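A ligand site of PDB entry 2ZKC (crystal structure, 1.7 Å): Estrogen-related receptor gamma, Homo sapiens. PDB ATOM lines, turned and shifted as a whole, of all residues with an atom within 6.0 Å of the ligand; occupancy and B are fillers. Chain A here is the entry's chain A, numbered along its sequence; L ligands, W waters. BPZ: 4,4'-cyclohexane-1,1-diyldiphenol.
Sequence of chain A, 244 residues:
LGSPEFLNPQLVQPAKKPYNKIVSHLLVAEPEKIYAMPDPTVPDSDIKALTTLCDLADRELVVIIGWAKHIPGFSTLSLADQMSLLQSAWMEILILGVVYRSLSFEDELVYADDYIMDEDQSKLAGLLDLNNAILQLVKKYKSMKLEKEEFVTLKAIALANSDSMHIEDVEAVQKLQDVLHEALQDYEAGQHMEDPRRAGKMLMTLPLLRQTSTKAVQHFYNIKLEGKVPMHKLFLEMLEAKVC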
ATOM      1  N   LEU A  50     -29.323  24.183  21.887  1.00  0.00           N
ATOM      2  CA  LEU A  50     -28.060  23.741  21.308  1.00  0.00           C
ATOM      3  C   LEU A  50     -26.854  24.400  21.961  1.00  0.00           C
ATOM      4  O   LEU A  50     -25.818  23.760  22.148  1.00  0.00           O
ATOM      5  CB  LEU A  50     -28.060  23.934  19.779  1.00  0.00           C
ATOM      6  CG  LEU A  50     -29.119  23.096  19.039  1.00  0.00           C
ATOM      7  CD1 LEU A  50     -29.285  23.656  17.617  1.00  0.00           C
ATOM      8  CD2 LEU A  50     -28.786  21.583  18.976  1.00  0.00           C
ATOM      9  N   LEU A  53     -26.344  22.745  25.332  1.00  0.00           N
ATOM     10  CA  LEU A  53     -25.791  21.374  25.113  1.00  0.00           C
ATOM     11  C   LEU A  53     -24.334  21.376  24.697  1.00  0.00           C
ATOM     12  O   LEU A  53     -23.543  20.560  25.216  1.00  0.00           O
ATOM     13  CB  LEU A  53     -26.632  20.626  24.084  1.00  0.00           C
ATOM     14  CG  LEU A  53     -27.984  20.193  24.618  1.00  0.00           C
ATOM     15  CD1 LEU A  53     -28.815  19.616  23.461  1.00  0.00           C
ATOM     16  CD2 LEU A  53     -27.826  19.168  25.708  1.00  0.00           C
ATOM     17  N   CYS A  54     -23.959  22.268  23.776  1.00  0.00           N
ATOM     18  CA  CYS A  54     -22.546  22.351  23.353  1.00  0.00           C
ATOM     19  C   CYS A  54     -21.650  22.879  24.477  1.00  0.00           C
ATOM     20  O   CYS A  54     -20.494  22.509  24.578  1.00  0.00           O
ATOM     21  CB  CYS A  54     -22.391  23.196  22.094  1.00  0.00           C
ATOM     22  SG  CYS A  54     -23.127  22.401  20.668  1.00  0.00           S
ATOM     23  N   LEU A  56     -22.246  22.363  27.700  1.00  0.00           N
ATOM     24  CA  LEU A  56     -22.142  21.248  28.624  1.00  0.00           C
ATOM     25  C   LEU A  56     -21.107  20.274  28.072  1.00  0.00           C
ATOM     26  O   LEU A  56     -20.234  19.830  28.836  1.00  0.00           O
ATOM     27  CB  LEU A  56     -23.486  20.514  28.760  1.00  0.00           C
ATOM     28  CG  LEU A  56     -23.553  19.244  29.601  1.00  0.00           C
ATOM     29  CD1 LEU A  56     -23.186  19.494  31.095  1.00  0.00           C
ATOM     30  CD2 LEU A  56     -24.942  18.600  29.531  1.00  0.00           C
ATOM     31  N   ALA A  57     -21.209  19.931  26.787  1.00  0.00           N
ATOM     32  CA  ALA A  57     -20.192  19.041  26.160  1.00  0.00           C
ATOM     33  C   ALA A  57     -18.754  19.566  26.343  1.00  0.00           C
ATOM     34  O   ALA A  57     -17.848  18.818  26.683  1.00  0.00           O
ATOM     35  CB  ALA A  57     -20.488  18.796  24.694  1.00  0.00           C
ATOM     36  N   GLU A  60     -17.707  18.876  29.850  1.00  0.00           N
ATOM     37  CA  GLU A  60     -17.527  17.431  30.020  1.00  0.00           C
ATOM     38  C   GLU A  60     -16.257  16.948  29.356  1.00  0.00           C
ATOM     39  O   GLU A  60     -15.629  16.018  29.870  1.00  0.00           O
ATOM     40  CB  GLU A  60     -18.713  16.674  29.459  1.00  0.00           C
ATOM     41  CG  GLU A  60     -19.935  16.797  30.313  1.00  0.00           C
ATOM     42  CD  GLU A  60     -20.878  15.664  30.063  1.00  0.00           C
ATOM     43  OE1 GLU A  60     -20.424  14.507  30.197  1.00  0.00           O
ATOM     44  OE2 GLU A  60     -22.041  15.926  29.726  1.00  0.00           O
ATOM     45  N   TRP A  90     -14.446  10.747  21.931  1.00  0.00           N
ATOM     46  CA  TRP A  90     -15.117  11.647  22.878  1.00  0.00           C
ATOM     47  C   TRP A  90     -16.651  11.632  22.785  1.00  0.00           C
ATOM     48  O   TRP A  90     -17.315  11.613  23.821  1.00  0.00           O
ATOM     49  CB  TRP A  90     -14.595  13.089  22.749  1.00  0.00           C
ATOM     50  CG  TRP A  90     -14.866  13.686  21.422  1.00  0.00           C
ATOM     51  CD1 TRP A  90     -14.125  13.531  20.286  1.00  0.00           C
ATOM     52  CD2 TRP A  90     -15.964  14.565  21.070  1.00  0.00           C
ATOM     53  NE1 TRP A  90     -14.691  14.241  19.240  1.00  0.00           N
ATOM     54  CE2 TRP A  90     -15.809  14.890  19.699  1.00  0.00           C
ATOM     55  CE3 TRP A  90     -17.045  15.114  21.773  1.00  0.00           C
ATOM     56  CZ2 TRP A  90     -16.721  15.726  19.022  1.00  0.00           C
ATOM     57  CZ3 TRP A  90     -17.941  15.959  21.102  1.00  0.00           C
ATOM     58  CH2 TRP A  90     -17.763  16.261  19.740  1.00  0.00           C
ATOM     59  N   MET A  91     -17.182  11.592  21.564  1.00  0.00           N
ATOM     60  CA  MET A  91     -18.638  11.614  21.403  1.00  0.00           C
ATOM     61  C   MET A  91     -19.269  10.341  21.975  1.00  0.00           C
ATOM     62  O   MET A  91     -20.324  10.378  22.616  1.00  0.00           O
ATOM     63  CB  MET A  91     -19.007  11.803  19.923  1.00  0.00           C
ATOM     64  CG  MET A  91     -20.500  11.873  19.693  1.00  0.00           C
ATOM     65  SD  MET A  91     -21.309  13.356  20.349  1.00  0.00           S
ATOM     66  CE  MET A  91     -20.900  14.438  18.991  1.00  0.00           C
ATOM     67  N   LEU A  94     -19.286  10.735  25.752  1.00  0.00           N
ATOM     68  CA  LEU A  94     -20.355  11.661  26.177  1.00  0.00           C
ATOM     69  C   LEU A  94     -21.719  10.955  26.072  1.00  0.00           C
ATOM     70  O   LEU A  94     -22.514  11.001  27.004  1.00  0.00           O
ATOM     71  CB  LEU A  94     -20.342  12.894  25.281  1.00  0.00           C
ATOM     72  CG  LEU A  94     -19.232  13.929  25.462  1.00  0.00           C
ATOM     73  CD1 LEU A  94     -19.440  15.026  24.458  1.00  0.00           C
ATOM     74  CD2 LEU A  94     -19.289  14.493  26.896  1.00  0.00           C
ATOM     75  N   ILE A  95     -21.970  10.274  24.953  1.00  0.00           N
ATOM     76  CA  ILE A  95     -23.265   9.640  24.746  1.00  0.00           C
ATOM     77  C   ILE A  95     -23.504   8.505  25.773  1.00  0.00           C
ATOM     78  O   ILE A  95     -24.581   8.382  26.361  1.00  0.00           O
ATOM     79  CB  ILE A  95     -23.433   9.178  23.274  1.00  0.00           C
ATOM     80  CG1 ILE A  95     -23.557  10.420  22.373  1.00  0.00           C
ATOM     81  CG2 ILE A  95     -24.671   8.244  23.149  1.00  0.00           C
ATOM     82  CD1 ILE A  95     -23.641  10.114  20.858  1.00  0.00           C
ATOM     83  N   GLY A  97     -22.488   8.355  28.710  1.00  0.00           N
ATOM     84  CA  GLY A  97     -22.872   9.067  29.950  1.00  0.00           C
ATOM     85  C   GLY A  97     -24.350   9.430  30.034  1.00  0.00           C
ATOM     86  O   GLY A  97     -25.039   9.061  30.993  1.00  0.00           O
ATOM     87  N   VAL A  98     -24.865  10.130  29.028  1.00  0.00           N
ATOM     88  CA  VAL A  98     -26.291  10.488  29.047  1.00  0.00           C
ATOM     89  C   VAL A  98     -27.216   9.249  29.004  1.00  0.00           C
ATOM     90  O   VAL A  98     -28.284   9.248  29.609  1.00  0.00           O
ATOM     91  CB  VAL A  98     -26.673  11.545  27.984  1.00  0.00           C
ATOM     92  CG1 VAL A  98     -26.461  11.016  26.571  1.00  0.00           C
ATOM     93  CG2 VAL A  98     -28.107  12.039  28.170  1.00  0.00           C
ATOM     94  N   ARG A 101     -27.199   7.892  32.584  1.00  0.00           N
ATOM     95  CA  ARG A 101     -27.946   8.747  33.512  1.00  0.00           C
ATOM     96  C   ARG A 101     -29.439   8.626  33.279  1.00  0.00           C
ATOM     97  O   ARG A 101     -30.230   8.985  34.146  1.00  0.00           O
ATOM     98  CB  ARG A 101     -27.538  10.192  33.360  1.00  0.00           C
ATOM     99  CG  ARG A 101     -26.096  10.457  33.828  1.00  0.00           C
ATOM    100  CD  ARG A 101     -25.811  11.948  33.865  1.00  0.00           C
ATOM    101  NE  ARG A 101     -25.740  12.583  32.537  1.00  0.00           N
ATOM    102  CZ  ARG A 101     -24.690  12.608  31.722  1.00  0.00           C
ATOM    103  NH1 ARG A 101     -23.546  11.949  32.001  1.00  0.00           N
ATOM    104  NH2 ARG A 101     -24.789  13.273  30.569  1.00  0.00           N
ATOM    105  N   LEU A 109     -34.118  12.024  28.230  1.00  0.00           N
ATOM    106  CA  LEU A 109     -32.655  11.960  28.306  1.00  0.00           C
ATOM    107  C   LEU A 109     -32.093  12.926  29.331  1.00  0.00           C
ATOM    108  O   LEU A 109     -32.268  14.139  29.209  1.00  0.00           O
ATOM    109  CB  LEU A 109     -32.049  12.261  26.937  1.00  0.00           C
ATOM    110  CG  LEU A 109     -32.393  11.185  25.893  1.00  0.00           C
ATOM    111  CD1 LEU A 109     -31.812  11.658  24.614  1.00  0.00           C
ATOM    112  CD2 LEU A 109     -31.799   9.807  26.309  1.00  0.00           C
ATOM    113  N   TYR A 111     -29.349  14.720  30.264  1.00  0.00           N
ATOM    114  CA  TYR A 111     -28.054  15.346  29.937  1.00  0.00           C
ATOM    115  C   TYR A 111     -27.367  15.825  31.204  1.00  0.00           C
ATOM    116  O   TYR A 111     -26.152  15.699  31.359  1.00  0.00           O
ATOM    117  CB  TYR A 111     -28.221  16.474  28.908  1.00  0.00           C
ATOM    118  CG  TYR A 111     -28.486  15.898  27.540  1.00  0.00           C
ATOM    119  CD1 TYR A 111     -29.788  15.695  27.088  1.00  0.00           C
ATOM    120  CD2 TYR A 111     -27.432  15.479  26.743  1.00  0.00           C
ATOM    121  CE1 TYR A 111     -30.011  15.137  25.841  1.00  0.00           C
ATOM    122  CE2 TYR A 111     -27.653  14.899  25.490  1.00  0.00           C
ATOM    123  CZ  TYR A 111     -28.945  14.746  25.065  1.00  0.00           C
ATOM    124  OH  TYR A 111     -29.157  14.157  23.833  1.00  0.00           O
ATOM    125  N   MET A 117     -34.256  16.165  28.704  1.00  0.00           N
ATOM    126  CA  MET A 117     -35.001  16.386  27.464  1.00  0.00           C
ATOM    127  C   MET A 117     -36.053  15.307  27.196  1.00  0.00           C
ATOM    128  O   MET A 117     -35.734  14.115  27.098  1.00  0.00           O
ATOM    129  CB  MET A 117     -34.066  16.534  26.257  1.00  0.00           C
ATOM    130  CG  MET A 117     -32.985  17.621  26.373  1.00  0.00           C
ATOM    131  SD  MET A 117     -32.063  17.813  24.846  1.00  0.00           S
ATOM    132  CE  MET A 117     -33.320  18.545  23.831  1.00  0.00           C
ATOM    133  N   LEU A 127     -33.344  17.781  17.347  1.00  0.00           N
ATOM    134  CA  LEU A 127     -32.611  16.562  17.702  1.00  0.00           C
ATOM    135  C   LEU A 127     -33.487  15.322  17.849  1.00  0.00           C
ATOM    136  O   LEU A 127     -33.065  14.349  18.488  1.00  0.00           O
ATOM    137  CB  LEU A 127     -31.839  16.776  19.014  1.00  0.00           C
ATOM    138  CG  LEU A 127     -30.827  17.918  19.037  1.00  0.00           C
ATOM    139  CD1 LEU A 127     -30.325  18.180  20.477  1.00  0.00           C
ATOM    140  CD2 LEU A 127     -29.664  17.641  18.092  1.00  0.00           C
ATOM    141  N   LEU A 130     -31.816  12.094  16.374  1.00  0.00           N
ATOM    142  CA  LEU A 130     -30.593  11.772  17.089  1.00  0.00           C
ATOM    143  C   LEU A 130     -30.920  11.287  18.482  1.00  0.00           C
ATOM    144  O   LEU A 130     -30.471  10.231  18.922  1.00  0.00           O
ATOM    145  CB  LEU A 130     -29.748  13.037  17.176  1.00  0.00           C
ATOM    146  CG  LEU A 130     -28.257  12.888  17.372  1.00  0.00           C
ATOM    147  CD1 LEU A 130     -27.684  11.718  16.514  1.00  0.00           C
ATOM    148  CD2 LEU A 130     -27.653  14.233  16.985  1.00  0.00           C
ATOM    149  N   ASN A 131     -31.750  12.054  19.187  1.00  0.00           N
ATOM    150  CA  ASN A 131     -32.175  11.646  20.530  1.00  0.00           C
ATOM    151  C   ASN A 131     -32.955  10.338  20.528  1.00  0.00           C
ATOM    152  O   ASN A 131     -32.867   9.555  21.473  1.00  0.00           O
ATOM    153  CB  ASN A 131     -32.928  12.776  21.220  1.00  0.00           C
ATOM    154  CG  ASN A 131     -31.970  13.796  21.855  1.00  0.00           C
ATOM    155  OD1 ASN A 131     -30.764  13.614  21.799  1.00  0.00           O
ATOM    156  ND2 ASN A 131     -32.502  14.844  22.439  1.00  0.00           N
ATOM    157  N   ILE A 134     -30.351   7.685  20.677  1.00  0.00           N
ATOM    158  CA  ILE A 134     -29.858   7.571  22.036  1.00  0.00           C
ATOM    159  C   ILE A 134     -30.867   6.821  22.909  1.00  0.00           C
ATOM    160  O   ILE A 134     -30.492   5.994  23.709  1.00  0.00           O
ATOM    161  CB  ILE A 134     -29.493   8.964  22.614  1.00  0.00           C
ATOM    162  CG1 ILE A 134     -28.426   9.611  21.712  1.00  0.00           C
ATOM    163  CG2 ILE A 134     -29.020   8.864  24.100  1.00  0.00           C
ATOM    164  CD1 ILE A 134     -27.963  11.038  22.173  1.00  0.00           C
ATOM    165  N   ALA A 216     -24.110  11.840  15.334  1.00  0.00           N
ATOM    166  CA  ALA A 216     -24.076  13.039  16.179  1.00  0.00           C
ATOM    167  C   ALA A 216     -22.949  13.980  15.760  1.00  0.00           C
ATOM    168  O   ALA A 216     -23.120  15.193  15.725  1.00  0.00           O
ATOM    169  CB  ALA A 216     -23.937  12.670  17.642  1.00  0.00           C
ATOM    170  N   PHE A 220     -23.602  17.870  14.465  1.00  0.00           N
ATOM    171  CA  PHE A 220     -23.041  19.056  15.097  1.00  0.00           C
ATOM    172  C   PHE A 220     -21.976  19.728  14.256  1.00  0.00           C
ATOM    173  O   PHE A 220     -21.742  20.917  14.405  1.00  0.00           O
ATOM    174  CB  PHE A 220     -22.629  18.792  16.543  1.00  0.00           C
ATOM    175  CG  PHE A 220     -23.798  18.701  17.451  1.00  0.00           C
ATOM    176  CD1 PHE A 220     -24.443  17.476  17.673  1.00  0.00           C
ATOM    177  CD2 PHE A 220     -24.327  19.862  18.017  1.00  0.00           C
ATOM    178  CE1 PHE A 220     -25.582  17.420  18.481  1.00  0.00           C
ATOM    179  CE2 PHE A 220     -25.456  19.804  18.805  1.00  0.00           C
ATOM    180  CZ  PHE A 220     -26.080  18.580  19.032  1.00  0.00           C
ATOM    181  N   PHE A 235     -14.353  22.020  22.488  1.00  0.00           N
ATOM    182  CA  PHE A 235     -15.408  21.329  21.740  1.00  0.00           C
ATOM    183  C   PHE A 235     -15.169  21.464  20.245  1.00  0.00           C
ATOM    184  O   PHE A 235     -15.260  20.489  19.497  1.00  0.00           O
ATOM    185  CB  PHE A 235     -16.800  21.862  22.139  1.00  0.00           C
ATOM    186  CG  PHE A 235     -17.942  21.226  21.378  1.00  0.00           C
ATOM    187  CD1 PHE A 235     -18.414  19.969  21.733  1.00  0.00           C
ATOM    188  CD2 PHE A 235     -18.523  21.884  20.292  1.00  0.00           C
ATOM    189  CE1 PHE A 235     -19.450  19.367  21.026  1.00  0.00           C
ATOM    190  CE2 PHE A 235     -19.560  21.282  19.584  1.00  0.00           C
ATOM    191  CZ  PHE A 235     -20.036  20.021  19.959  1.00  0.00           C
HETATM  192  O2  BPZ L   1     -28.198  13.701  20.353  1.00  0.00           O
HETATM  193  C16 BPZ L   1     -27.221  14.367  21.024  1.00  0.00           C
HETATM  194  C15 BPZ L   1     -25.909  13.959  20.870  1.00  0.00           C
HETATM  195  C14 BPZ L   1     -24.893  14.636  21.552  1.00  0.00           C
HETATM  196  C17 BPZ L   1     -27.541  15.441  21.842  1.00  0.00           C
HETATM  197  C18 BPZ L   1     -26.531  16.125  22.526  1.00  0.00           C
HETATM  198  C7  BPZ L   1     -25.189  15.723  22.380  1.00  0.00           C
HETATM  199  C5  BPZ L   1     -24.077  16.453  23.109  1.00  0.00           C
HETATM  200  C8  BPZ L   1     -22.715  16.271  22.426  1.00  0.00           C
HETATM  201  C1  BPZ L   1     -22.559  17.042  21.113  1.00  0.00           C
HETATM  202  C4  BPZ L   1     -24.375  17.961  23.188  1.00  0.00           C
HETATM  203  C3  BPZ L   1     -24.297  18.666  21.829  1.00  0.00           C
HETATM  204  C2  BPZ L   1     -22.894  18.519  21.239  1.00  0.00           C
HETATM  205  C6  BPZ L   1     -23.884  15.893  24.494  1.00  0.00           C
HETATM  206  C13 BPZ L   1     -23.993  14.519  24.710  1.00  0.00           C
HETATM  207  C12 BPZ L   1     -23.791  13.961  25.970  1.00  0.00           C
HETATM  208  C11 BPZ L   1     -23.453  14.801  27.038  1.00  0.00           C
HETATM  209  O1  BPZ L   1     -23.244  14.262  28.283  1.00  0.00           O
HETATM  210  C10 BPZ L   1     -23.329  16.181  26.837  1.00  0.00           C
HETATM  211  C9  BPZ L   1     -23.548  16.730  25.571  1.00  0.00           C
HETATM  212  O   HOH W   1     -21.732  12.250  29.630  1.00  0.00           O
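O1 of the ligand sits at hydrogen-bond distance from NH2 of Arg 101, at 2.9 Å. The side-chain amide oxygen (OD1) of Asn 131 sits at hydrogen-bond distance from an oxygen (O2) of the ligand. The side-chain carboxylate of Glu 60 sits at hydrogen-bond distance from an oxygen (O1) of the ligand.
Merely in contact with the ligand: Tyr 111, Leu 130, Ile 134, Phe 220, Leu 94, Leu 53, Phe 235, Met 91, Ala 57, Cys 54, Leu 56 and Ala 216. Hydrophobic or aromatic side chains that line the ligand: Leu 53, Leu 56, Ala 57, Met 91, Leu 94, Tyr 111, Leu 130, Ile 134, Ala 216, Phe 220 and Phe 235. Within 4 Å of the ligand: Leu 53, Cys 54, Leu 56, Ala 57, Glu 60, Met 91, Leu 94, Arg 101, Tyr 111, Leu 130, Asn 131, Ile 134, Ala 216, Phe 220 and Phe 235. The nearest printed residue that does not touch the ligand is Val 98 (4.02 Å).
Water W1 lies within hydrogen-bond range of OE1 of Glu 60 (2.7 Å), O1 of the ligand (2.9 Å), NH1 of Arg 101 (3.0 Å) and O of Leu 94 (3.0 Å).
O of Tyr 111 lies within hydrogen-bond range of NH2 of Arg 101, at 2.9 Å. The guanidinium group (NH1) of Arg 101 sits close to the backbone carbonyl oxygen (O) of Gly 97 (3.4 Å). SG of Cys 54 is in hydrogen-bond range of O of Leu 50 (3.4 Å). The side-chain hydroxyl of Tyr 111 lies within hydrogen-bond range of the side-chain amide oxygen of Asn 131 (2.6 Å). The guanidinium group of Arg 101 is in salt-bridge range of the side-chain carboxylate of Glu 60.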
